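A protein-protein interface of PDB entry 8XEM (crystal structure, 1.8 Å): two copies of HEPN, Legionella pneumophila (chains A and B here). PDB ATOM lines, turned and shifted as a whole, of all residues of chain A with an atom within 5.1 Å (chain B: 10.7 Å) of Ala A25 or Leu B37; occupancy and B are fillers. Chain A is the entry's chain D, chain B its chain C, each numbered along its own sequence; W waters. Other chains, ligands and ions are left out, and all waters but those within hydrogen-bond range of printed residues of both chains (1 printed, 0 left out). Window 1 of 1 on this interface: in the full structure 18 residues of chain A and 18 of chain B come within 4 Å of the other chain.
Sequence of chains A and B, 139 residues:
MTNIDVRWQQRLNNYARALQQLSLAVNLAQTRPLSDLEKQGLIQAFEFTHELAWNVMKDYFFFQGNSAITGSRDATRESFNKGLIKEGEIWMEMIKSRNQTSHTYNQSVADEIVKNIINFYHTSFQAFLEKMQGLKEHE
Of the 14 printed residues of chain A, 6 touch a printed residue of chain B. Hydrophobic or aromatic side chains of chain A that line the printed part of chain B: Ala A25 and Leu A37. Of the 23 printed residues of chain B, 7 touch a printed residue of chain A. Along chain B the printed residues that touch a printed residue of chain A span positions 25 to 105. Among the printed residues, 11 pairs touch across the chains. Among the printed residues, no Asp or Glu carboxylate lies within 4 Å of a Lys or Arg side-chain nitrogen of the other chain.
Ala A25 touches one residue of chain B. Leu B37 touches just these residues of chain A: Ala A25 (3.8 Å), Glu A38 (3.8 Å), Gly A41 (3.4 Å) and Leu A42 (3.5 Å). Of chain B, only Leu B37 comes within 4 Å of Glu A38. Of chain B, only Leu B37, Gln B40 and Gly B41 come within 4 Å of Gly A41. Of the printed residues of chain A, Leu B42 touches Leu A37. Printed residues of chain A within 4 Å of Glu B38: Leu A37 (3.8 Å). The nearest printed residue of chain A that does not touch Gly B41 is Glu A38 (5.6 Å).
Ala A25 touches Leu B37, and with the chains exchanged Leu A37 touches Ala B25. Leu A37 touches Glu B38, and with the chains exchanged Glu A38 touches Leu B37. Leu A37 touches Gly B41, and with the chains exchanged Gly A41 touches Leu B37. Leu A37 touches Leu B42, and with the chains exchanged Leu A42 touches Leu B37. Positions printed for both chains: 25, 28, 34, 37, 38, 41 and 42. Of the 11 pairs that touch across the chains among the printed residues, 9 have their exchanged pair printed and touching as well.
Water W1 bridges OG of Ser B35 (2.6 Å) and OE2 of Glu A38 (2.7 Å).
NE2 of Gln A21 sits at hydrogen-bond distance from O of Tyr B105.
NE2 of Gln B40 sits at hydrogen-bond distance from O of Thr B104, at 2.8 Å. N of Ser B35 is in hydrogen-bond range of OE1 of Glu B38. The side-chain hydroxyl (OG) of Ser B35 lies close to the backbone NH (N) of Leu B37 (3.5 Å). OE2 of Glu B38 is in salt-bridge range of NH2 of Arg B32 (2.7 Å).
Ala A25 touches Leu B37 (CB to CD1, 3.8 Å). CD1 of Leu A37 touches CB of Ala B25 (3.7 Å). Leu A37 touches Glu B38. Leu A37 touches Gly B41. Leu B42 touches Leu A37. Leu B37 touches Glu A38. C of Gly A41 touches CD1 of Leu B37 (3.4 Å). CA of Gly A41 touches C of Gln B40, 3.7 Å away. CA of Gly B41 touches N of Gly A41, 3.3 Å away. Leu B37 touches Leu A42.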
ATOM      1  N   GLN A  21      -7.212  -1.954 -17.143  1.00  0.00           N
ATOM      2  CA  GLN A  21      -6.459  -1.542 -15.964  1.00  0.00           C
ATOM      3  C   GLN A  21      -7.368  -0.900 -14.927  1.00  0.00           C
ATOM      4  O   GLN A  21      -7.217  -1.143 -13.725  1.00  0.00           O
ATOM      5  CB  GLN A  21      -5.351  -0.574 -16.359  1.00  0.00           C
ATOM      6  CG  GLN A  21      -4.214  -1.223 -17.103  1.00  0.00           C
ATOM      7  CD  GLN A  21      -3.302  -0.205 -17.741  1.00  0.00           C
ATOM      8  OE1 GLN A  21      -2.665   0.592 -17.052  1.00  0.00           O
ATOM      9  NE2 GLN A  21      -3.239  -0.215 -19.068  1.00  0.00           N
ATOM     10  N   LEU A  22      -8.309  -0.067 -15.369  1.00  0.00           N
ATOM     11  CA  LEU A  22      -9.287   0.484 -14.439  1.00  0.00           C
ATOM     12  C   LEU A  22     -10.071  -0.629 -13.753  1.00  0.00           C
ATOM     13  O   LEU A  22     -10.269  -0.600 -12.533  1.00  0.00           O
ATOM     14  CB  LEU A  22     -10.225   1.436 -15.176  1.00  0.00           C
ATOM     15  CG  LEU A  22     -11.382   1.982 -14.344  1.00  0.00           C
ATOM     16  CD1 LEU A  22     -10.802   2.728 -13.161  1.00  0.00           C
ATOM     17  CD2 LEU A  22     -12.259   2.890 -15.176  1.00  0.00           C
ATOM     18  N   SER A  23     -10.525  -1.621 -14.526  1.00  0.00           N
ATOM     19  CA  SER A  23     -11.303  -2.716 -13.955  1.00  0.00           C
ATOM     20  C   SER A  23     -10.528  -3.440 -12.863  1.00  0.00           C
ATOM     21  O   SER A  23     -11.109  -3.859 -11.852  1.00  0.00           O
ATOM     22  CB  SER A  23     -11.711  -3.705 -15.049  1.00  0.00           C
ATOM     23  OG  SER A  23     -12.682  -3.139 -15.906  1.00  0.00           O
ATOM     24  N   LEU A  24      -9.221  -3.622 -13.053  1.00  0.00           N
ATOM     25  CA  LEU A  24      -8.423  -4.270 -12.018  1.00  0.00           C
ATOM     26  C   LEU A  24      -8.547  -3.515 -10.704  1.00  0.00           C
ATOM     27  O   LEU A  24      -8.779  -4.109  -9.643  1.00  0.00           O
ATOM     28  CB  LEU A  24      -6.961  -4.352 -12.446  1.00  0.00           C
ATOM     29  CG  LEU A  24      -6.607  -5.431 -13.464  1.00  0.00           C
ATOM     30  CD1 LEU A  24      -5.198  -5.163 -13.995  1.00  0.00           C
ATOM     31  CD2 LEU A  24      -6.702  -6.837 -12.888  1.00  0.00           C
ATOM     32  N   ALA A  25      -8.407  -2.192 -10.765  1.00  0.00           N
ATOM     33  CA  ALA A  25      -8.450  -1.372  -9.563  1.00  0.00           C
ATOM     34  C   ALA A  25      -9.855  -1.320  -8.976  1.00  0.00           C
ATOM     35  O   ALA A  25     -10.021  -1.353  -7.750  1.00  0.00           O
ATOM     36  CB  ALA A  25      -7.940   0.030  -9.895  1.00  0.00           C
ATOM     37  N   VAL A  26     -10.879  -1.250  -9.831  1.00  0.00           N
ATOM     38  CA  VAL A  26     -12.256  -1.231  -9.346  1.00  0.00           C
ATOM     39  C   VAL A  26     -12.582  -2.535  -8.633  1.00  0.00           C
ATOM     40  O   VAL A  26     -13.204  -2.539  -7.564  1.00  0.00           O
ATOM     41  CB  VAL A  26     -13.230  -0.979 -10.514  1.00  0.00           C
ATOM     42  CG1 VAL A  26     -14.671  -1.255 -10.089  1.00  0.00           C
ATOM     43  CG2 VAL A  26     -13.090   0.431 -11.041  1.00  0.00           C
ATOM     44  N   ASN A  27     -12.191  -3.665  -9.221  1.00  0.00           N
ATOM     45  CA  ASN A  27     -12.484  -4.940  -8.579  1.00  0.00           C
ATOM     46  C   ASN A  27     -11.681  -5.099  -7.298  1.00  0.00           C
ATOM     47  O   ASN A  27     -12.152  -5.730  -6.347  1.00  0.00           O
ATOM     48  CB  ASN A  27     -12.223  -6.086  -9.550  1.00  0.00           C
ATOM     49  CG  ASN A  27     -13.266  -6.152 -10.652  1.00  0.00           C
ATOM     50  OD1 ASN A  27     -12.941  -6.314 -11.827  1.00  0.00           O
ATOM     51  ND2 ASN A  27     -14.532  -6.009 -10.272  1.00  0.00           N
ATOM     52  N   LEU A  28     -10.486  -4.505  -7.241  1.00  0.00           N
ATOM     53  CA  LEU A  28      -9.716  -4.531  -6.004  1.00  0.00           C
ATOM     54  C   LEU A  28     -10.421  -3.744  -4.908  1.00  0.00           C
ATOM     55  O   LEU A  28     -10.456  -4.175  -3.750  1.00  0.00           O
ATOM     56  CB  LEU A  28      -8.319  -3.970  -6.247  1.00  0.00           C
ATOM     57  CG  LEU A  28      -7.365  -4.033  -5.055  1.00  0.00           C
ATOM     58  CD1 LEU A  28      -7.044  -5.479  -4.711  1.00  0.00           C
ATOM     59  CD2 LEU A  28      -6.101  -3.249  -5.358  1.00  0.00           C
ATOM     60  N   ALA A  29     -10.994  -2.589  -5.255  1.00  0.00           N
ATOM     61  CA  ALA A  29     -11.669  -1.767  -4.257  1.00  0.00           C
ATOM     62  C   ALA A  29     -12.907  -2.458  -3.698  1.00  0.00           C
ATOM     63  O   ALA A  29     -13.271  -2.224  -2.541  1.00  0.00           O
ATOM     64  CB  ALA A  29     -12.038  -0.410  -4.857  1.00  0.00           C
ATOM     65  N   LEU A  34      -8.907   0.855  -0.295  1.00  0.00           N
ATOM     66  CA  LEU A  34      -7.720   1.324  -0.987  1.00  0.00           C
ATOM     67  C   LEU A  34      -6.955   2.280  -0.084  1.00  0.00           C
ATOM     68  O   LEU A  34      -7.550   3.046   0.681  1.00  0.00           O
ATOM     69  CB  LEU A  34      -8.091   2.022  -2.292  1.00  0.00           C
ATOM     70  CG  LEU A  34      -8.868   1.181  -3.299  1.00  0.00           C
ATOM     71  CD1 LEU A  34      -9.058   1.990  -4.568  1.00  0.00           C
ATOM     72  CD2 LEU A  34      -8.159  -0.112  -3.601  1.00  0.00           C
ATOM     73  N   LEU A  37      -2.963   6.478  -1.625  1.00  0.00           N
ATOM     74  CA  LEU A  37      -2.259   6.487  -2.903  1.00  0.00           C
ATOM     75  C   LEU A  37      -2.994   5.658  -3.949  1.00  0.00           C
ATOM     76  O   LEU A  37      -3.071   6.053  -5.117  1.00  0.00           O
ATOM     77  CB  LEU A  37      -0.834   5.972  -2.707  1.00  0.00           C
ATOM     78  CG  LEU A  37       0.159   6.092  -3.863  1.00  0.00           C
ATOM     79  CD1 LEU A  37       0.310   7.538  -4.286  1.00  0.00           C
ATOM     80  CD2 LEU A  37       1.508   5.489  -3.458  1.00  0.00           C
ATOM     81  N   GLU A  38      -3.542   4.505  -3.561  1.00  0.00           N
ATOM     82  CA  GLU A  38      -4.281   3.701  -4.531  1.00  0.00           C
ATOM     83  C   GLU A  38      -5.529   4.430  -5.016  1.00  0.00           C
ATOM     84  O   GLU A  38      -5.899   4.329  -6.192  1.00  0.00           O
ATOM     85  CB  GLU A  38      -4.644   2.345  -3.929  1.00  0.00           C
ATOM     86  CG  GLU A  38      -3.447   1.415  -3.770  1.00  0.00           C
ATOM     87  CD  GLU A  38      -3.752   0.183  -2.928  1.00  0.00           C
ATOM     88  OE1 GLU A  38      -4.573   0.286  -1.994  1.00  0.00           O
ATOM     89  OE2 GLU A  38      -3.163  -0.886  -3.198  1.00  0.00           O
ATOM     90  N   GLY A  41      -4.526   6.572  -7.679  1.00  0.00           N
ATOM     91  CA  GLY A  41      -4.293   5.786  -8.880  1.00  0.00           C
ATOM     92  C   GLY A  41      -5.577   5.404  -9.586  1.00  0.00           C
ATOM     93  O   GLY A  41      -5.645   5.412 -10.818  1.00  0.00           O
ATOM     94  N   LEU A  42      -6.609   5.044  -8.821  1.00  0.00           N
ATOM     95  CA  LEU A  42      -7.911   4.778  -9.422  1.00  0.00           C
ATOM     96  C   LEU A  42      -8.431   6.009 -10.150  1.00  0.00           C
ATOM     97  O   LEU A  42      -8.965   5.909 -11.261  1.00  0.00           O
ATOM     98  CB  LEU A  42      -8.899   4.336  -8.346  1.00  0.00           C
ATOM     99  CG  LEU A  42     -10.322   4.017  -8.802  1.00  0.00           C
ATOM    100  CD1 LEU A  42     -10.323   2.861  -9.788  1.00  0.00           C
ATOM    101  CD2 LEU A  42     -11.202   3.691  -7.609  1.00  0.00           C
ATOM    102  N   ALA B  25       4.224   9.517  -0.879  1.00  0.00           N
ATOM    103  CA  ALA B  25       4.372   8.506  -1.928  1.00  0.00           C
ATOM    104  C   ALA B  25       5.839   8.309  -2.315  1.00  0.00           C
ATOM    105  O   ALA B  25       6.285   7.177  -2.546  1.00  0.00           O
ATOM    106  CB  ALA B  25       3.541   8.884  -3.153  1.00  0.00           C
ATOM    107  N   LEU B  28       7.549   6.278   0.424  1.00  0.00           N
ATOM    108  CA  LEU B  28       7.114   4.888   0.328  1.00  0.00           C
ATOM    109  C   LEU B  28       7.830   4.187  -0.817  1.00  0.00           C
ATOM    110  O   LEU B  28       8.232   3.023  -0.692  1.00  0.00           O
ATOM    111  CB  LEU B  28       5.598   4.828   0.155  1.00  0.00           C
ATOM    112  CG  LEU B  28       4.945   3.465  -0.030  1.00  0.00           C
ATOM    113  CD1 LEU B  28       3.786   3.288   0.930  1.00  0.00           C
ATOM    114  CD2 LEU B  28       4.450   3.339  -1.454  1.00  0.00           C
ATOM    115  N   ARG B  32      10.050   0.511  -0.890  1.00  0.00           N
ATOM    116  CA  ARG B  32       9.751  -0.728  -1.597  1.00  0.00           C
ATOM    117  C   ARG B  32       9.256  -0.378  -2.991  1.00  0.00           C
ATOM    118  O   ARG B  32       8.935   0.786  -3.271  1.00  0.00           O
ATOM    119  CB  ARG B  32       8.701  -1.561  -0.842  1.00  0.00           C
ATOM    120  CG  ARG B  32       7.427  -0.785  -0.537  1.00  0.00           C
ATOM    121  CD  ARG B  32       6.232  -1.704  -0.413  1.00  0.00           C
ATOM    122  NE  ARG B  32       5.001  -0.975  -0.135  1.00  0.00           N
ATOM    123  CZ  ARG B  32       4.200  -0.475  -1.068  1.00  0.00           C
ATOM    124  NH1 ARG B  32       4.503  -0.550  -2.352  1.00  0.00           N
ATOM    125  NH2 ARG B  32       3.067   0.116  -0.700  1.00  0.00           N
ATOM    126  N   PRO B  33       9.174  -1.360  -3.887  1.00  0.00           N
ATOM    127  CA  PRO B  33       8.629  -1.082  -5.223  1.00  0.00           C
ATOM    128  C   PRO B  33       7.153  -0.723  -5.151  1.00  0.00           C
ATOM    129  O   PRO B  33       6.401  -1.266  -4.337  1.00  0.00           O
ATOM    130  CB  PRO B  33       8.851  -2.394  -5.989  1.00  0.00           C
ATOM    131  CG  PRO B  33       9.879  -3.154  -5.183  1.00  0.00           C
ATOM    132  CD  PRO B  33       9.638  -2.753  -3.754  1.00  0.00           C
ATOM    133  N   LEU B  34       6.745   0.200  -6.017  1.00  0.00           N
ATOM    134  CA  LEU B  34       5.350   0.594  -6.127  1.00  0.00           C
ATOM    135  C   LEU B  34       4.612  -0.345  -7.073  1.00  0.00           C
ATOM    136  O   LEU B  34       5.156  -0.764  -8.099  1.00  0.00           O
ATOM    137  CB  LEU B  34       5.222   2.023  -6.655  1.00  0.00           C
ATOM    138  CG  LEU B  34       5.859   3.165  -5.875  1.00  0.00           C
ATOM    139  CD1 LEU B  34       5.406   4.499  -6.433  1.00  0.00           C
ATOM    140  CD2 LEU B  34       5.493   3.076  -4.427  1.00  0.00           C
ATOM    141  N   SER B  35       3.365  -0.656  -6.731  1.00  0.00           N
ATOM    142  CA  SER B  35       2.481  -1.360  -7.648  1.00  0.00           C
ATOM    143  C   SER B  35       2.130  -0.458  -8.829  1.00  0.00           C
ATOM    144  O   SER B  35       2.329   0.758  -8.793  1.00  0.00           O
ATOM    145  CB  SER B  35       1.209  -1.800  -6.926  1.00  0.00           C
ATOM    146  OG  SER B  35       0.352  -0.695  -6.695  1.00  0.00           O
ATOM    147  N   ASP B  36       1.597  -1.066  -9.891  1.00  0.00           N
ATOM    148  CA  ASP B  36       1.190  -0.269 -11.048  1.00  0.00           C
ATOM    149  C   ASP B  36       0.154   0.782 -10.651  1.00  0.00           C
ATOM    150  O   ASP B  36       0.199   1.932 -11.116  1.00  0.00           O
ATOM    151  CB  ASP B  36       0.634  -1.179 -12.147  1.00  0.00           C
ATOM    152  CG  ASP B  36       1.719  -1.958 -12.879  1.00  0.00           C
ATOM    153  OD1 ASP B  36       2.919  -1.702 -12.649  1.00  0.00           O
ATOM    154  OD2 ASP B  36       1.365  -2.830 -13.698  1.00  0.00           O
ATOM    155  N   LEU B  37      -0.787   0.403  -9.786  1.00  0.00           N
ATOM    156  CA  LEU B  37      -1.815   1.341  -9.342  1.00  0.00           C
ATOM    157  C   LEU B  37      -1.211   2.439  -8.480  1.00  0.00           C
ATOM    158  O   LEU B  37      -1.600   3.611  -8.579  1.00  0.00           O
ATOM    159  CB  LEU B  37      -2.894   0.583  -8.573  1.00  0.00           C
ATOM    160  CG  LEU B  37      -4.075   1.381  -8.020  1.00  0.00           C
ATOM    161  CD1 LEU B  37      -4.798   2.106  -9.148  1.00  0.00           C
ATOM    162  CD2 LEU B  37      -5.012   0.466  -7.238  1.00  0.00           C
ATOM    163  N   GLU B  38      -0.249   2.077  -7.632  1.00  0.00           N
ATOM    164  CA  GLU B  38       0.418   3.068  -6.801  1.00  0.00           C
ATOM    165  C   GLU B  38       1.230   4.041  -7.650  1.00  0.00           C
ATOM    166  O   GLU B  38       1.312   5.231  -7.326  1.00  0.00           O
ATOM    167  CB  GLU B  38       1.306   2.362  -5.780  1.00  0.00           C
ATOM    168  CG  GLU B  38       0.549   1.769  -4.592  1.00  0.00           C
ATOM    169  CD  GLU B  38       1.463   0.986  -3.663  1.00  0.00           C
ATOM    170  OE1 GLU B  38       2.430   0.379  -4.165  1.00  0.00           O
ATOM    171  OE2 GLU B  38       1.235   0.997  -2.434  1.00  0.00           O
ATOM    172  N   LYS B  39       1.838   3.558  -8.739  1.00  0.00           N
ATOM    173  CA  LYS B  39       2.509   4.470  -9.663  1.00  0.00           C
ATOM    174  C   LYS B  39       1.520   5.439 -10.296  1.00  0.00           C
ATOM    175  O   LYS B  39       1.807   6.637 -10.434  1.00  0.00           O
ATOM    176  CB  LYS B  39       3.239   3.692 -10.757  1.00  0.00           C
ATOM    177  CG  LYS B  39       4.516   3.024 -10.299  1.00  0.00           C
ATOM    178  CD  LYS B  39       5.143   2.223 -11.427  1.00  0.00           C
ATOM    179  CE  LYS B  39       6.520   1.706 -11.044  1.00  0.00           C
ATOM    180  NZ  LYS B  39       6.997   0.702 -12.039  1.00  0.00           N
ATOM    181  N   GLN B  40       0.359   4.931 -10.725  1.00  0.00           N
ATOM    182  CA  GLN B  40      -0.679   5.835 -11.217  1.00  0.00           C
ATOM    183  C   GLN B  40      -1.030   6.885 -10.160  1.00  0.00           C
ATOM    184  O   GLN B  40      -1.268   8.058 -10.481  1.00  0.00           O
ATOM    185  CB  GLN B  40      -1.919   5.037 -11.615  1.00  0.00           C
ATOM    186  CG  GLN B  40      -1.694   4.049 -12.761  1.00  0.00           C
ATOM    187  CD  GLN B  40      -1.199   4.698 -14.042  1.00  0.00           C
ATOM    188  OE1 GLN B  40      -1.385   5.896 -14.262  1.00  0.00           O
ATOM    189  NE2 GLN B  40      -0.573   3.901 -14.900  1.00  0.00           N
ATOM    190  N   GLY B  41      -1.067   6.478  -8.890  1.00  0.00           N
ATOM    191  CA  GLY B  41      -1.376   7.429  -7.832  1.00  0.00           C
ATOM    192  C   GLY B  41      -0.300   8.483  -7.647  1.00  0.00           C
ATOM    193  O   GLY B  41      -0.600   9.654  -7.391  1.00  0.00           O
ATOM    194  N   LEU B  42       0.967   8.078  -7.740  1.00  0.00           N
ATOM    195  CA  LEU B  42       2.052   9.051  -7.674  1.00  0.00           C
ATOM    196  C   LEU B  42       1.941  10.044  -8.824  1.00  0.00           C
ATOM    197  O   LEU B  42       2.181  11.243  -8.649  1.00  0.00           O
ATOM    198  CB  LEU B  42       3.403   8.338  -7.692  1.00  0.00           C
ATOM    199  CG  LEU B  42       4.643   9.234  -7.633  1.00  0.00           C
ATOM    200  CD1 LEU B  42       4.719  10.008  -6.331  1.00  0.00           C
ATOM    201  CD2 LEU B  42       5.900   8.391  -7.821  1.00  0.00           C
ATOM    202  N   ILE B  43       1.527   9.568  -9.999  1.00  0.00           N
ATOM    203  CA  ILE B  43       1.360  10.467 -11.140  1.00  0.00           C
ATOM    204  C   ILE B  43       0.238  11.474 -10.875  1.00  0.00           C
ATOM    205  O   ILE B  43       0.390  12.672 -11.136  1.00  0.00           O
ATOM    206  CB  ILE B  43       1.117   9.651 -12.421  1.00  0.00           C
ATOM    207  CG1 ILE B  43       2.391   8.886 -12.794  1.00  0.00           C
ATOM    208  CG2 ILE B  43       0.694  10.549 -13.566  1.00  0.00           C
ATOM    209  CD1 ILE B  43       2.170   7.729 -13.737  1.00  0.00           C
ATOM    210  N   GLN B  44      -0.905  11.007 -10.357  1.00  0.00           N
ATOM    211  CA  GLN B  44      -1.985  11.938 -10.008  1.00  0.00           C
ATOM    212  C   GLN B  44      -1.533  12.955  -8.960  1.00  0.00           C
ATOM    213  O   GLN B  44      -1.858  14.149  -9.056  1.00  0.00           O
ATOM    214  CB  GLN B  44      -3.211  11.160  -9.515  1.00  0.00           C
ATOM    215  CG  GLN B  44      -4.383  11.992  -8.945  1.00  0.00           C
ATOM    216  CD  GLN B  44      -4.978  12.985  -9.928  1.00  0.00           C
ATOM    217  OE1 GLN B  44      -4.706  12.929 -11.124  1.00  0.00           O
ATOM    218  NE2 GLN B  44      -5.805  13.896  -9.423  1.00  0.00           N
ATOM    219  N   ALA B  45      -0.803  12.505  -7.936  1.00  0.00           N
ATOM    220  CA  ALA B  45      -0.305  13.453  -6.941  1.00  0.00           C
ATOM    221  C   ALA B  45       0.623  14.475  -7.587  1.00  0.00           C
ATOM    222  O   ALA B  45       0.592  15.664  -7.243  1.00  0.00           O
ATOM    223  CB  ALA B  45       0.407  12.713  -5.808  1.00  0.00           C
ATOM    224  N   GLU B  47       0.298  15.517 -10.609  1.00  0.00           N
ATOM    225  CA  GLU B  47      -0.578  16.418 -11.357  1.00  0.00           C
ATOM    226  C   GLU B  47      -1.171  17.497 -10.449  1.00  0.00           C
ATOM    227  O   GLU B  47      -1.148  18.690 -10.790  1.00  0.00           O
ATOM    228  CB  GLU B  47      -1.691  15.632 -12.049  1.00  0.00           C
ATOM    229  CG  GLU B  47      -1.237  14.731 -13.197  1.00  0.00           C
ATOM    230  CD  GLU B  47      -2.385  13.898 -13.754  1.00  0.00           C
ATOM    231  OE1 GLU B  47      -3.446  14.471 -14.070  1.00  0.00           O
ATOM    232  OE2 GLU B  47      -2.248  12.659 -13.827  1.00  0.00           O
ATOM    233  N   THR B 104      -0.571   7.202 -19.577  1.00  0.00           N
ATOM    234  CA  THR B 104       0.041   6.333 -18.576  1.00  0.00           C
ATOM    235  C   THR B 104      -0.638   4.973 -18.486  1.00  0.00           C
ATOM    236  O   THR B 104      -0.209   4.132 -17.688  1.00  0.00           O
ATOM    237  CB  THR B 104       0.064   7.004 -17.197  1.00  0.00           C
ATOM    238  OG1 THR B 104      -1.266   7.280 -16.750  1.00  0.00           O
ATOM    239  CG2 THR B 104       0.860   8.299 -17.256  1.00  0.00           C
ATOM    240  N   TYR B 105      -1.666   4.716 -19.291  1.00  0.00           N
ATOM    241  CA  TYR B 105      -2.104   3.336 -19.429  1.00  0.00           C
ATOM    242  C   TYR B 105      -1.060   2.483 -20.140  1.00  0.00           C
ATOM    243  O   TYR B 105      -1.180   1.254 -20.130  1.00  0.00           O
ATOM    244  CB  TYR B 105      -3.437   3.268 -20.166  1.00  0.00           C
ATOM    245  CG  TYR B 105      -3.392   3.780 -21.579  1.00  0.00           C
ATOM    246  CD1 TYR B 105      -3.587   5.125 -21.858  1.00  0.00           C
ATOM    247  CD2 TYR B 105      -3.163   2.915 -22.640  1.00  0.00           C
ATOM    248  CE1 TYR B 105      -3.550   5.593 -23.155  1.00  0.00           C
ATOM    249  CE2 TYR B 105      -3.123   3.375 -23.940  1.00  0.00           C
ATOM    250  CZ  TYR B 105      -3.319   4.714 -24.193  1.00  0.00           C
ATOM    251  OH  TYR B 105      -3.279   5.176 -25.489  1.00  0.00           O
ATOM    252  N   GLN B 107       2.644   1.208 -19.732  1.00  0.00           N
ATOM    253  CA  GLN B 107       3.539   1.111 -18.582  1.00  0.00           C
ATOM    254  C   GLN B 107       4.836   1.879 -18.802  1.00  0.00           C
ATOM    255  O   GLN B 107       5.412   2.393 -17.841  1.00  0.00           O
ATOM    256  CB  GLN B 107       3.837  -0.359 -18.275  1.00  0.00           C
ATOM    257  CG  GLN B 107       4.254  -0.669 -16.825  1.00  0.00           C
ATOM    258  CD  GLN B 107       3.519   0.155 -15.779  1.00  0.00           C
ATOM    259  OE1 GLN B 107       2.307   0.352 -15.866  1.00  0.00           O
ATOM    260  NE2 GLN B 107       4.254   0.651 -14.788  1.00  0.00           N
ATOM    261  N   ALA B 110       4.147   5.522 -17.945  1.00  0.00           N
ATOM    262  CA  ALA B 110       3.972   5.632 -16.501  1.00  0.00           C
ATOM    263  C   ALA B 110       5.318   5.567 -15.789  1.00  0.00           C
ATOM    264  O   ALA B 110       5.607   6.380 -14.904  1.00  0.00           O
ATOM    265  CB  ALA B 110       3.037   4.531 -15.996  1.00  0.00           C
ATOM    266  N   ASP B 111       6.161   4.607 -16.171  1.00  0.00           N
ATOM    267  CA  ASP B 111       7.442   4.451 -15.492  1.00  0.00           C
ATOM    268  C   ASP B 111       8.336   5.665 -15.714  1.00  0.00           C
ATOM    269  O   ASP B 111       9.038   6.096 -14.795  1.00  0.00           O
ATOM    270  CB  ASP B 111       8.144   3.181 -15.971  1.00  0.00           C
ATOM    271  CG  ASP B 111       7.479   1.921 -15.460  1.00  0.00           C
ATOM    272  OD1 ASP B 111       6.616   2.019 -14.561  1.00  0.00           O
ATOM    273  OD2 ASP B 111       7.822   0.831 -15.960  1.00  0.00           O
ATOM    274  N   VAL B 114       7.006   8.526 -13.508  1.00  0.00           N
ATOM    275  CA  VAL B 114       7.327   8.202 -12.119  1.00  0.00           C
ATOM    276  C   VAL B 114       8.801   8.464 -11.841  1.00  0.00           C
ATOM    277  O   VAL B 114       9.170   9.046 -10.812  1.00  0.00           O
ATOM    278  CB  VAL B 114       6.947   6.739 -11.821  1.00  0.00           C
ATOM    279  CG1 VAL B 114       7.590   6.261 -10.529  1.00  0.00           C
ATOM    280  CG2 VAL B 114       5.432   6.587 -11.761  1.00  0.00           C
HETATM  281  O   HOH W   1      -1.705  -1.622  -5.388  1.00  0.00           O
